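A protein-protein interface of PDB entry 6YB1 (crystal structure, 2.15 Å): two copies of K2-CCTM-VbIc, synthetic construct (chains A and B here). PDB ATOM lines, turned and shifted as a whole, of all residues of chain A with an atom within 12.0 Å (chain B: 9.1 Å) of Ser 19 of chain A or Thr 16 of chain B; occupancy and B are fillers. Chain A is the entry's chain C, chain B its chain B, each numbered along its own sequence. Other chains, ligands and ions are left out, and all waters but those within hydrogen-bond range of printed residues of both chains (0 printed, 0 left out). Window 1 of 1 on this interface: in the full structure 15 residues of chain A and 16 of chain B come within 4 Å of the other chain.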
ATOM      1  N   THR A   9      11.379 -10.711  30.903  1.00  0.00           N
ATOM      2  CA  THR A   9      10.160 -11.437  31.247  1.00  0.00           C
ATOM      3  C   THR A   9       9.343 -11.769  30.002  1.00  0.00           C
ATOM      4  O   THR A   9       8.906 -12.914  29.814  1.00  0.00           O
ATOM      5  CB  THR A   9       9.334 -10.608  32.233  1.00  0.00           C
ATOM      6  OG1 THR A   9      10.131 -10.313  33.387  1.00  0.00           O
ATOM      7  CG2 THR A   9       8.092 -11.370  32.661  1.00  0.00           C
ATOM      8  N   VAL A  10       9.128 -10.773  29.138  1.00  0.00           N
ATOM      9  CA  VAL A  10       8.373 -11.012  27.907  1.00  0.00           C
ATOM     10  C   VAL A  10       9.050 -12.081  27.056  1.00  0.00           C
ATOM     11  O   VAL A  10       8.395 -12.988  26.516  1.00  0.00           O
ATOM     12  CB  VAL A  10       8.204  -9.701  27.122  1.00  0.00           C
ATOM     13  CG1 VAL A  10       7.553  -9.987  25.781  1.00  0.00           C
ATOM     14  CG2 VAL A  10       7.383  -8.706  27.924  1.00  0.00           C
ATOM     15  N   ILE A  11      10.370 -11.988  26.909  1.00  0.00           N
ATOM     16  CA  ILE A  11      11.074 -12.920  26.042  1.00  0.00           C
ATOM     17  C   ILE A  11      11.117 -14.310  26.666  1.00  0.00           C
ATOM     18  O   ILE A  11      11.056 -15.310  25.950  1.00  0.00           O
ATOM     19  CB  ILE A  11      12.460 -12.343  25.696  1.00  0.00           C
ATOM     20  CG1 ILE A  11      12.254 -11.032  24.938  1.00  0.00           C
ATOM     21  CG2 ILE A  11      13.287 -13.292  24.835  1.00  0.00           C
ATOM     22  CD1 ILE A  11      13.425 -10.136  24.938  1.00  0.00           C
ATOM     23  N   SER A  12      11.197 -14.406  27.997  1.00  0.00           N
ATOM     24  CA  SER A  12      11.111 -15.706  28.655  1.00  0.00           C
ATOM     25  C   SER A  12       9.754 -16.353  28.423  1.00  0.00           C
ATOM     26  O   SER A  12       9.669 -17.566  28.210  1.00  0.00           O
ATOM     27  CB  SER A  12      11.372 -15.571  30.155  1.00  0.00           C
ATOM     28  OG  SER A  12      12.690 -15.135  30.406  1.00  0.00           O
ATOM     29  N   ALA A  13       8.676 -15.569  28.480  1.00  0.00           N
ATOM     30  CA  ALA A  13       7.363 -16.138  28.180  1.00  0.00           C
ATOM     31  C   ALA A  13       7.292 -16.623  26.733  1.00  0.00           C
ATOM     32  O   ALA A  13       6.742 -17.702  26.449  1.00  0.00           O
ATOM     33  CB  ALA A  13       6.269 -15.108  28.455  1.00  0.00           C
ATOM     34  N   LEU A  14       7.877 -15.853  25.807  1.00  0.00           N
ATOM     35  CA  LEU A  14       7.930 -16.289  24.415  1.00  0.00           C
ATOM     36  C   LEU A  14       8.734 -17.577  24.267  1.00  0.00           C
ATOM     37  O   LEU A  14       8.329 -18.493  23.541  1.00  0.00           O
ATOM     38  CB  LEU A  14       8.531 -15.183  23.545  1.00  0.00           C
ATOM     39  CG  LEU A  14       8.542 -15.474  22.044  1.00  0.00           C
ATOM     40  CD1 LEU A  14       7.136 -15.728  21.547  1.00  0.00           C
ATOM     41  CD2 LEU A  14       9.172 -14.327  21.277  1.00  0.00           C
ATOM     42  N   ALA A  15       9.889 -17.652  24.933  1.00  0.00           N
ATOM     43  CA  ALA A  15      10.708 -18.859  24.906  1.00  0.00           C
ATOM     44  C   ALA A  15       9.939 -20.044  25.462  1.00  0.00           C
ATOM     45  O   ALA A  15      10.065 -21.161  24.958  1.00  0.00           O
ATOM     46  CB  ALA A  15      12.004 -18.645  25.689  1.00  0.00           C
ATOM     47  N   THR A  16       9.147 -19.818  26.515  1.00  0.00           N
ATOM     48  CA  THR A  16       8.344 -20.893  27.089  1.00  0.00           C
ATOM     49  C   THR A  16       7.356 -21.427  26.062  1.00  0.00           C
ATOM     50  O   THR A  16       7.219 -22.648  25.883  1.00  0.00           O
ATOM     51  CB  THR A  16       7.604 -20.368  28.324  1.00  0.00           C
ATOM     52  OG1 THR A  16       8.556 -19.909  29.290  1.00  0.00           O
ATOM     53  CG2 THR A  16       6.718 -21.450  28.955  1.00  0.00           C
ATOM     54  N   VAL A  17       6.700 -20.522  25.336  1.00  0.00           N
ATOM     55  CA  VAL A  17       5.746 -20.955  24.320  1.00  0.00           C
ATOM     56  C   VAL A  17       6.447 -21.708  23.190  1.00  0.00           C
ATOM     57  O   VAL A  17       5.978 -22.762  22.736  1.00  0.00           O
ATOM     58  CB  VAL A  17       4.971 -19.745  23.784  1.00  0.00           C
ATOM     59  CG1 VAL A  17       4.048 -20.179  22.665  1.00  0.00           C
ATOM     60  CG2 VAL A  17       4.192 -19.092  24.912  1.00  0.00           C
ATOM     61  N   ILE A  18       7.586 -21.188  22.725  1.00  0.00           N
ATOM     62  CA  ILE A  18       8.279 -21.817  21.603  1.00  0.00           C
ATOM     63  C   ILE A  18       8.871 -23.158  22.019  1.00  0.00           C
ATOM     64  O   ILE A  18       8.897 -24.109  21.231  1.00  0.00           O
ATOM     65  CB  ILE A  18       9.348 -20.878  21.027  1.00  0.00           C
ATOM     66  CG1 ILE A  18       8.700 -19.586  20.533  1.00  0.00           C
ATOM     67  CG2 ILE A  18      10.062 -21.549  19.862  1.00  0.00           C
ATOM     68  CD1 ILE A  18       7.562 -19.822  19.568  1.00  0.00           C
ATOM     69  N   SER A  19       9.372 -23.253  23.251  1.00  0.00           N
ATOM     70  CA  SER A  19       9.888 -24.520  23.759  1.00  0.00           C
ATOM     71  C   SER A  19       8.774 -25.557  23.876  1.00  0.00           C
ATOM     72  O   SER A  19       8.989 -26.745  23.609  1.00  0.00           O
ATOM     73  CB  SER A  19      10.571 -24.293  25.106  1.00  0.00           C
ATOM     74  OG  SER A  19      11.150 -25.487  25.582  1.00  0.00           O
ATOM     75  N   ALA A  20       7.575 -25.126  24.271  1.00  0.00           N
ATOM     76  CA  ALA A  20       6.445 -26.047  24.291  1.00  0.00           C
ATOM     77  C   ALA A  20       6.111 -26.530  22.885  1.00  0.00           C
ATOM     78  O   ALA A  20       5.857 -27.723  22.667  1.00  0.00           O
ATOM     79  CB  ALA A  20       5.230 -25.369  24.926  1.00  0.00           C
ATOM     80  N   LEU A  21       6.125 -25.613  21.913  1.00  0.00           N
ATOM     81  CA  LEU A  21       5.890 -26.001  20.524  1.00  0.00           C
ATOM     82  C   LEU A  21       6.948 -26.985  20.034  1.00  0.00           C
ATOM     83  O   LEU A  21       6.632 -27.955  19.330  1.00  0.00           O
ATOM     84  CB  LEU A  21       5.875 -24.758  19.638  1.00  0.00           C
ATOM     85  CG  LEU A  21       5.763 -24.998  18.134  1.00  0.00           C
ATOM     86  CD1 LEU A  21       4.424 -25.610  17.786  1.00  0.00           C
ATOM     87  CD2 LEU A  21       5.985 -23.709  17.359  1.00  0.00           C
ATOM     88  N   ALA A  22       8.214 -26.729  20.372  1.00  0.00           N
ATOM     89  CA  ALA A  22       9.296 -27.643  20.023  1.00  0.00           C
ATOM     90  C   ALA A  22       9.069 -29.015  20.642  1.00  0.00           C
ATOM     91  O   ALA A  22       9.316 -30.041  19.999  1.00  0.00           O
ATOM     92  CB  ALA A  22      10.640 -27.054  20.460  1.00  0.00           C
ATOM     93  N   THR A  23       8.579 -29.051  21.885  1.00  0.00           N
ATOM     94  CA  THR A  23       8.271 -30.323  22.535  1.00  0.00           C
ATOM     95  C   THR A  23       7.213 -31.086  21.745  1.00  0.00           C
ATOM     96  O   THR A  23       7.339 -32.294  21.504  1.00  0.00           O
ATOM     97  CB  THR A  23       7.767 -30.073  23.961  1.00  0.00           C
ATOM     98  OG1 THR A  23       8.741 -29.335  24.700  1.00  0.00           O
ATOM     99  CG2 THR A  23       7.493 -31.387  24.683  1.00  0.00           C
ATOM    100  N   VAL A  24       6.162 -30.384  21.319  1.00  0.00           N
ATOM    101  CA  VAL A  24       5.086 -31.057  20.595  1.00  0.00           C
ATOM    102  C   VAL A  24       5.571 -31.564  19.240  1.00  0.00           C
ATOM    103  O   VAL A  24       5.251 -32.687  18.827  1.00  0.00           O
ATOM    104  CB  VAL A  24       3.877 -30.118  20.460  1.00  0.00           C
ATOM    105  CG1 VAL A  24       2.885 -30.659  19.441  1.00  0.00           C
ATOM    106  CG2 VAL A  24       3.206 -29.972  21.801  1.00  0.00           C
ATOM    107  N   ILE A  25       6.376 -30.768  18.538  1.00  0.00           N
ATOM    108  CA  ILE A  25       6.870 -31.206  17.236  1.00  0.00           C
ATOM    109  C   ILE A  25       7.859 -32.355  17.400  1.00  0.00           C
ATOM    110  O   ILE A  25       7.919 -33.268  16.568  1.00  0.00           O
ATOM    111  CB  ILE A  25       7.476 -30.016  16.476  1.00  0.00           C
ATOM    112  CG1 ILE A  25       6.388 -28.978  16.213  1.00  0.00           C
ATOM    113  CG2 ILE A  25       8.085 -30.465  15.163  1.00  0.00           C
ATOM    114  CD1 ILE A  25       6.887 -27.744  15.514  1.00  0.00           C
ATOM    115  N   SER A  26       8.628 -32.348  18.488  1.00  0.00           N
ATOM    116  CA  SER A  26       9.553 -33.439  18.762  1.00  0.00           C
ATOM    117  C   SER A  26       8.803 -34.730  19.069  1.00  0.00           C
ATOM    118  O   SER A  26       9.214 -35.812  18.637  1.00  0.00           O
ATOM    119  CB  SER A  26      10.472 -33.047  19.921  1.00  0.00           C
ATOM    120  OG  SER A  26      11.733 -33.672  19.809  1.00  0.00           O
ATOM    121  N   ALA A  27       7.692 -34.638  19.803  1.00  0.00           N
ATOM    122  CA  ALA A  27       6.857 -35.819  20.013  1.00  0.00           C
ATOM    123  C   ALA A  27       6.282 -36.321  18.691  1.00  0.00           C
ATOM    124  O   ALA A  27       6.243 -37.537  18.435  1.00  0.00           O
ATOM    125  CB  ALA A  27       5.742 -35.501  21.009  1.00  0.00           C
ATOM    126  N   TRP A  28       5.865 -35.391  17.824  1.00  0.00           N
ATOM    127  CA  TRP A  28       5.372 -35.757  16.498  1.00  0.00           C
ATOM    128  C   TRP A  28       6.432 -36.494  15.693  1.00  0.00           C
ATOM    129  O   TRP A  28       6.132 -37.485  15.019  1.00  0.00           O
ATOM    130  CB  TRP A  28       4.945 -34.496  15.748  1.00  0.00           C
ATOM    131  CG  TRP A  28       4.401 -34.731  14.375  1.00  0.00           C
ATOM    132  CD1 TRP A  28       3.587 -35.747  13.970  1.00  0.00           C
ATOM    133  CD2 TRP A  28       4.705 -33.965  13.202  1.00  0.00           C
ATOM    134  NE1 TRP A  28       3.329 -35.635  12.623  1.00  0.00           N
ATOM    135  CE2 TRP A  28       4.009 -34.553  12.128  1.00  0.00           C
ATOM    136  CE3 TRP A  28       5.487 -32.828  12.959  1.00  0.00           C
ATOM    137  CZ2 TRP A  28       4.070 -34.042  10.832  1.00  0.00           C
ATOM    138  CZ3 TRP A  28       5.546 -32.323  11.672  1.00  0.00           C
ATOM    139  CH2 TRP A  28       4.842 -32.930  10.626  1.00  0.00           C
ATOM    140  N   ALA B   8      14.842 -35.944  23.113  1.00  0.00           N
ATOM    141  CA  ALA B   8      14.687 -34.530  22.782  1.00  0.00           C
ATOM    142  C   ALA B   8      13.335 -34.008  23.253  1.00  0.00           C
ATOM    143  O   ALA B   8      13.233 -32.876  23.733  1.00  0.00           O
ATOM    144  CB  ALA B   8      14.869 -34.307  21.280  1.00  0.00           C
ATOM    145  N   THR B   9      12.290 -34.829  23.142  1.00  0.00           N
ATOM    146  CA  THR B   9      10.973 -34.421  23.622  1.00  0.00           C
ATOM    147  C   THR B   9      10.987 -34.189  25.127  1.00  0.00           C
ATOM    148  O   THR B   9      10.525 -33.148  25.616  1.00  0.00           O
ATOM    149  CB  THR B   9       9.942 -35.492  23.264  1.00  0.00           C
ATOM    150  OG1 THR B   9       9.934 -35.699  21.847  1.00  0.00           O
ATOM    151  CG2 THR B   9       8.543 -35.092  23.736  1.00  0.00           C
ATOM    152  N   VAL B  10      11.531 -35.152  25.876  1.00  0.00           N
ATOM    153  CA  VAL B  10      11.587 -35.025  27.332  1.00  0.00           C
ATOM    154  C   VAL B  10      12.366 -33.777  27.734  1.00  0.00           C
ATOM    155  O   VAL B  10      11.921 -32.980  28.575  1.00  0.00           O
ATOM    156  CB  VAL B  10      12.199 -36.291  27.953  1.00  0.00           C
ATOM    157  CG1 VAL B  10      12.401 -36.088  29.436  1.00  0.00           C
ATOM    158  CG2 VAL B  10      11.314 -37.506  27.687  1.00  0.00           C
ATOM    159  N   ILE B  11      13.533 -33.572  27.127  1.00  0.00           N
ATOM    160  CA  ILE B  11      14.369 -32.449  27.541  1.00  0.00           C
ATOM    161  C   ILE B  11      13.767 -31.122  27.099  1.00  0.00           C
ATOM    162  O   ILE B  11      13.888 -30.117  27.810  1.00  0.00           O
ATOM    163  CB  ILE B  11      15.810 -32.662  27.053  1.00  0.00           C
ATOM    164  CG1 ILE B  11      16.357 -33.917  27.739  1.00  0.00           C
ATOM    165  CG2 ILE B  11      16.674 -31.440  27.344  1.00  0.00           C
ATOM    166  CD1 ILE B  11      17.500 -34.538  27.067  1.00  0.00           C
ATOM    167  N   SER B  12      13.093 -31.084  25.949  1.00  0.00           N
ATOM    168  CA  SER B  12      12.383 -29.866  25.576  1.00  0.00           C
ATOM    169  C   SER B  12      11.298 -29.546  26.592  1.00  0.00           C
ATOM    170  O   SER B  12      11.101 -28.381  26.951  1.00  0.00           O
ATOM    171  CB  SER B  12      11.774 -30.005  24.184  1.00  0.00           C
ATOM    172  OG  SER B  12      12.775 -30.154  23.210  1.00  0.00           O
ATOM    173  N   ALA B  13      10.584 -30.568  27.075  1.00  0.00           N
ATOM    174  CA  ALA B  13       9.567 -30.321  28.097  1.00  0.00           C
ATOM    175  C   ALA B  13      10.192 -29.767  29.377  1.00  0.00           C
ATOM    176  O   ALA B  13       9.653 -28.835  29.993  1.00  0.00           O
ATOM    177  CB  ALA B  13       8.788 -31.606  28.381  1.00  0.00           C
ATOM    178  N   LEU B  14      11.353 -30.302  29.770  1.00  0.00           N
ATOM    179  CA  LEU B  14      12.046 -29.774  30.950  1.00  0.00           C
ATOM    180  C   LEU B  14      12.467 -28.324  30.735  1.00  0.00           C
ATOM    181  O   LEU B  14      12.403 -27.496  31.660  1.00  0.00           O
ATOM    182  CB  LEU B  14      13.258 -30.642  31.292  1.00  0.00           C
ATOM    183  CG  LEU B  14      12.929 -32.075  31.711  1.00  0.00           C
ATOM    184  CD1 LEU B  14      14.202 -32.857  31.999  1.00  0.00           C
ATOM    185  CD2 LEU B  14      11.982 -32.099  32.919  1.00  0.00           C
ATOM    186  N   ALA B  15      12.960 -28.018  29.532  1.00  0.00           N
ATOM    187  CA  ALA B  15      13.309 -26.648  29.189  1.00  0.00           C
ATOM    188  C   ALA B  15      12.093 -25.741  29.305  1.00  0.00           C
ATOM    189  O   ALA B  15      12.206 -24.599  29.764  1.00  0.00           O
ATOM    190  CB  ALA B  15      13.903 -26.595  27.781  1.00  0.00           C
ATOM    191  N   THR B  16      10.925 -26.234  28.883  1.00  0.00           N
ATOM    192  CA  THR B  16       9.688 -25.464  28.996  1.00  0.00           C
ATOM    193  C   THR B  16       9.361 -25.182  30.458  1.00  0.00           C
ATOM    194  O   THR B  16       8.937 -24.074  30.814  1.00  0.00           O
ATOM    195  CB  THR B  16       8.528 -26.223  28.338  1.00  0.00           C
ATOM    196  OG1 THR B  16       8.819 -26.469  26.954  1.00  0.00           O
ATOM    197  CG2 THR B  16       7.248 -25.420  28.433  1.00  0.00           C
ATOM    198  N   VAL B  17       9.564 -26.182  31.318  1.00  0.00           N
ATOM    199  CA  VAL B  17       9.271 -26.024  32.740  1.00  0.00           C
ATOM    200  C   VAL B  17      10.160 -24.948  33.349  1.00  0.00           C
ATOM    201  O   VAL B  17       9.687 -24.008  34.018  1.00  0.00           O
ATOM    202  CB  VAL B  17       9.468 -27.372  33.460  1.00  0.00           C
ATOM    203  CG1 VAL B  17       9.651 -27.181  34.972  1.00  0.00           C
ATOM    204  CG2 VAL B  17       8.320 -28.317  33.156  1.00  0.00           C
ATOM    205  N   ILE B  18      11.460 -25.029  33.062  1.00  0.00           N
ATOM    206  CA  ILE B  18      12.392 -24.074  33.641  1.00  0.00           C
ATOM    207  C   ILE B  18      12.167 -22.689  33.049  1.00  0.00           C
ATOM    208  O   ILE B  18      12.326 -21.683  33.742  1.00  0.00           O
ATOM    209  CB  ILE B  18      13.843 -24.561  33.465  1.00  0.00           C
ATOM    210  CG1 ILE B  18      14.026 -25.911  34.157  1.00  0.00           C
ATOM    211  CG2 ILE B  18      14.820 -23.572  34.065  1.00  0.00           C
ATOM    212  CD1 ILE B  18      13.584 -25.908  35.607  1.00  0.00           C
ATOM    213  N   SER B  19      11.808 -22.607  31.768  1.00  0.00           N
ATOM    214  CA  SER B  19      11.552 -21.312  31.155  1.00  0.00           C
ATOM    215  C   SER B  19      10.331 -20.639  31.770  1.00  0.00           C
ATOM    216  O   SER B  19      10.326 -19.418  31.960  1.00  0.00           O
ATOM    217  CB  SER B  19      11.404 -21.478  29.642  1.00  0.00           C
ATOM    218  OG  SER B  19      11.262 -20.225  29.006  1.00  0.00           O
ATOM    219  N   ALA B  20       9.285 -21.410  32.094  1.00  0.00           N
ATOM    220  CA  ALA B  20       8.135 -20.818  32.773  1.00  0.00           C
ATOM    221  C   ALA B  20       8.518 -20.296  34.157  1.00  0.00           C
ATOM    222  O   ALA B  20       8.095 -19.198  34.565  1.00  0.00           O
ATOM    223  CB  ALA B  20       7.002 -21.840  32.876  1.00  0.00           C
ATOM    224  N   LEU B  21       9.321 -21.068  34.897  1.00  0.00           N
ATOM    225  CA  LEU B  21       9.803 -20.573  36.187  1.00  0.00           C
ATOM    226  C   LEU B  21      10.666 -19.320  36.024  1.00  0.00           C
ATOM    227  O   LEU B  21      10.569 -18.378  36.823  1.00  0.00           O
ATOM    228  CB  LEU B  21      10.569 -21.672  36.916  1.00  0.00           C
ATOM    229  CG  LEU B  21       9.668 -22.838  37.327  1.00  0.00           C
ATOM    230  CD1 LEU B  21      10.478 -23.906  38.019  1.00  0.00           C
ATOM    231  CD2 LEU B  21       8.550 -22.353  38.240  1.00  0.00           C
ATOM    232  N   ALA B  22      11.541 -19.310  35.013  1.00  0.00           N
ATOM    233  CA  ALA B  22      12.364 -18.138  34.725  1.00  0.00           C
ATOM    234  C   ALA B  22      11.501 -16.927  34.421  1.00  0.00           C
ATOM    235  O   ALA B  22      11.827 -15.808  34.829  1.00  0.00           O
ATOM    236  CB  ALA B  22      13.310 -18.429  33.558  1.00  0.00           C
ATOM    237  N   THR B  23      10.400 -17.129  33.696  1.00  0.00           N
ATOM    238  CA  THR B  23       9.491 -16.028  33.402  1.00  0.00           C
ATOM    239  C   THR B  23       8.929 -15.445  34.690  1.00  0.00           C
ATOM    240  O   THR B  23       8.894 -14.218  34.872  1.00  0.00           O
ATOM    241  CB  THR B  23       8.349 -16.519  32.507  1.00  0.00           C
ATOM    242  OG1 THR B  23       8.882 -17.061  31.294  1.00  0.00           O
ATOM    243  CG2 THR B  23       7.396 -15.379  32.171  1.00  0.00           C
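Thr 9 of chain A touches Thr 23 of chain B, and with the chains exchanged Thr 23 of chain A touches Thr 9 of chain B. Ser 12 of chain A touches Thr 23 of chain B, and with the chains exchanged Thr 23 of chain A touches Ser 12 of chain B. Ala 15 of chain A touches Ser 19 of chain B, and with the chains exchanged Ser 19 of chain A touches Ala 15 of chain B. Thr 16 of chain B touches its own counterpart, Thr 16 of chain A. Positions printed for both chains: 9, 10, 11, 12, 13, 14, 15, 16, 17, 18, 19, 20, 21, 22 and 23. Of the 20 pairs that touch across the chains among the printed residues, 17 have their exchanged pair printed and touching as well.
Of the 16 printed residues of chain B, 9 touch a printed residue of chain A. Printed residues of chain B that touch a printed residue of chain A: Ala 8, Thr 9, Ser 12, Ala 13, Ala 15, Thr 16, Ser 19, Ala 20 and Thr 23. Hydrophobic or aromatic side chains of chain B within 4 Å of the printed part of chain A: Ala 8, Ala 13, Ala 15 and Ala 20. Of the 20 printed residues of chain A, 10 touch a printed residue of chain B. Among the printed residues, 20 pairs touch across the chains. Among the printed residues, no Asp or Glu carboxylate lies within 4 Å of a Lys or Arg side-chain nitrogen of the other chain.
Thr 16 of chain B touches just these residues of chain A: Thr 16 (3.8 Å), Ser 19 (2.9 Å), Ala 20 (3.2 Å) and Thr 23 (3.6 Å). Thr 16 of chain A touches four residues of chain B. Of chain B, only Thr 16 (3.2 Å) comes within 4 Å of Ala 20 of chain A. No residue of chain B comes within 4 Å of Ala 22 of chain A. Of the printed residues of chain A, Ser 12 of chain B touches Ser 19 (3.2 Å) and Thr 23 (3.1 Å). Ala 13 of chain B touches one residue of chain A. Of chain A, only Ser 19 (3.7 Å) comes within 4 Å of Ala 15 of chain B. Ser 19 of chain B touches just these residues of chain A: Ser 12 (3.2 Å), Ala 15 (3.7 Å) and Thr 16 (2.7 Å). Ala 20 of chain B touches just one residue of chain A: Thr 16 (3.3 Å). Printed residues of chain A within 4 Å of Ala 8 of chain B: Ser 26. Printed residues of chain A within 4 Å of Thr 23 of chain B: Thr 9 (3.7 Å), Ser 12 (3.1 Å), Ala 13 (3.2 Å) and Thr 16 (3.5 Å). Of the printed residues of chain B, Thr 9 of chain A touches Thr 23. Printed residues of chain B within 4 Å of Ser 26 of chain A: Ala 8 and Thr 9. The nearest residue of chain B that does not touch Ser 19 of chain A is Ala 13 of chain B (5.3 Å). The nearest printed residue of chain A that does not touch Thr 16 of chain B is Leu 21 of chain A (5.8 Å).
OG1 of Thr 9 of chain B sits close to O of Ser 26 of chain A (3.3 Å). The side-chain hydroxyl of Thr 9 of chain B lies within hydrogen-bond range of the backbone NH of Ala 27 of chain A. The backbone carbonyl oxygen of Ser 12 of chain B lies within hydrogen-bond range of the side-chain hydroxyl of Ser 19 of chain A, at 3.2 Å. O of Ser 12 of chain B lies close to OG1 of Thr 23 of chain A (3.4 Å). N of Ala 13 of chain B sits at hydrogen-bond distance from OG1 of Thr 23 of chain A (3.2 Å). The side-chain hydroxyl (OG1) of Thr 16 of chain B sits at hydrogen-bond distance from the side-chain hydroxyl (OG) of Ser 19 of chain A, at 2.9 Å. N of Ala 20 of chain A is in hydrogen-bond range of OG1 of Thr 16 of chain B, at 3.2 Å. O of Ser 12 of chain A lies within hydrogen-bond range of OG of Ser 19 of chain B, 3.2 Å away. The side-chain hydroxyl of Ser 19 of chain B lies within hydrogen-bond range of the side-chain hydroxyl of Thr 16 of chain A. The side-chain hydroxyl (OG1) of Thr 16 of chain A lies within hydrogen-bond range of the backbone NH (N) of Ala 20 of chain B. OG1 of Thr 23 of chain B lies close to O of Ser 12 of chain A, 3.2 Å away. N of Ala 13 of chain A sits at hydrogen-bond distance from OG1 of Thr 23 of chain B, 3.2 Å away. The side-chain hydroxyl (OG1) of Thr 16 of chain A lies within hydrogen-bond range of the side-chain hydroxyl (OG1) of Thr 23 of chain B, at 3.5 Å.
Among the printed residues, merely in contact across the chains: Ser 26 of chain A with Ala 8 of chain B, Thr 23 of chain A with Thr 9 of chain B, Thr 23 of chain A with Thr 16 of chain B, Ser 19 of chain A with Ala 15 of chain B, Thr 9 of chain A with Thr 23 of chain B, Ala 15 of chain A with Ser 19 of chain B and Thr 16 of chain A with Thr 16 of chain B.
The side-chain hydroxyl (OG) of Ser 12 of chain B is in hydrogen-bond range of the backbone carbonyl oxygen (O) of Ala 8 of chain B (2.8 Å). The backbone carbonyl oxygen (O) of Ser 12 of chain B sits at hydrogen-bond distance from the side-chain hydroxyl (OG1) of Thr 16 of chain B (3.0 Å). OG1 of Thr 23 of chain B is in hydrogen-bond range of O of Ser 19 of chain B, at 2.8 Å. The backbone carbonyl oxygen (O) of Ser 12 of chain A sits at hydrogen-bond distance from the side-chain hydroxyl (OG1) of Thr 16 of chain A (2.8 Å). The backbone carbonyl oxygen (O) of Ser 19 of chain A lies within hydrogen-bond range of the side-chain hydroxyl (OG1) of Thr 23 of chain A (2.8 Å).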
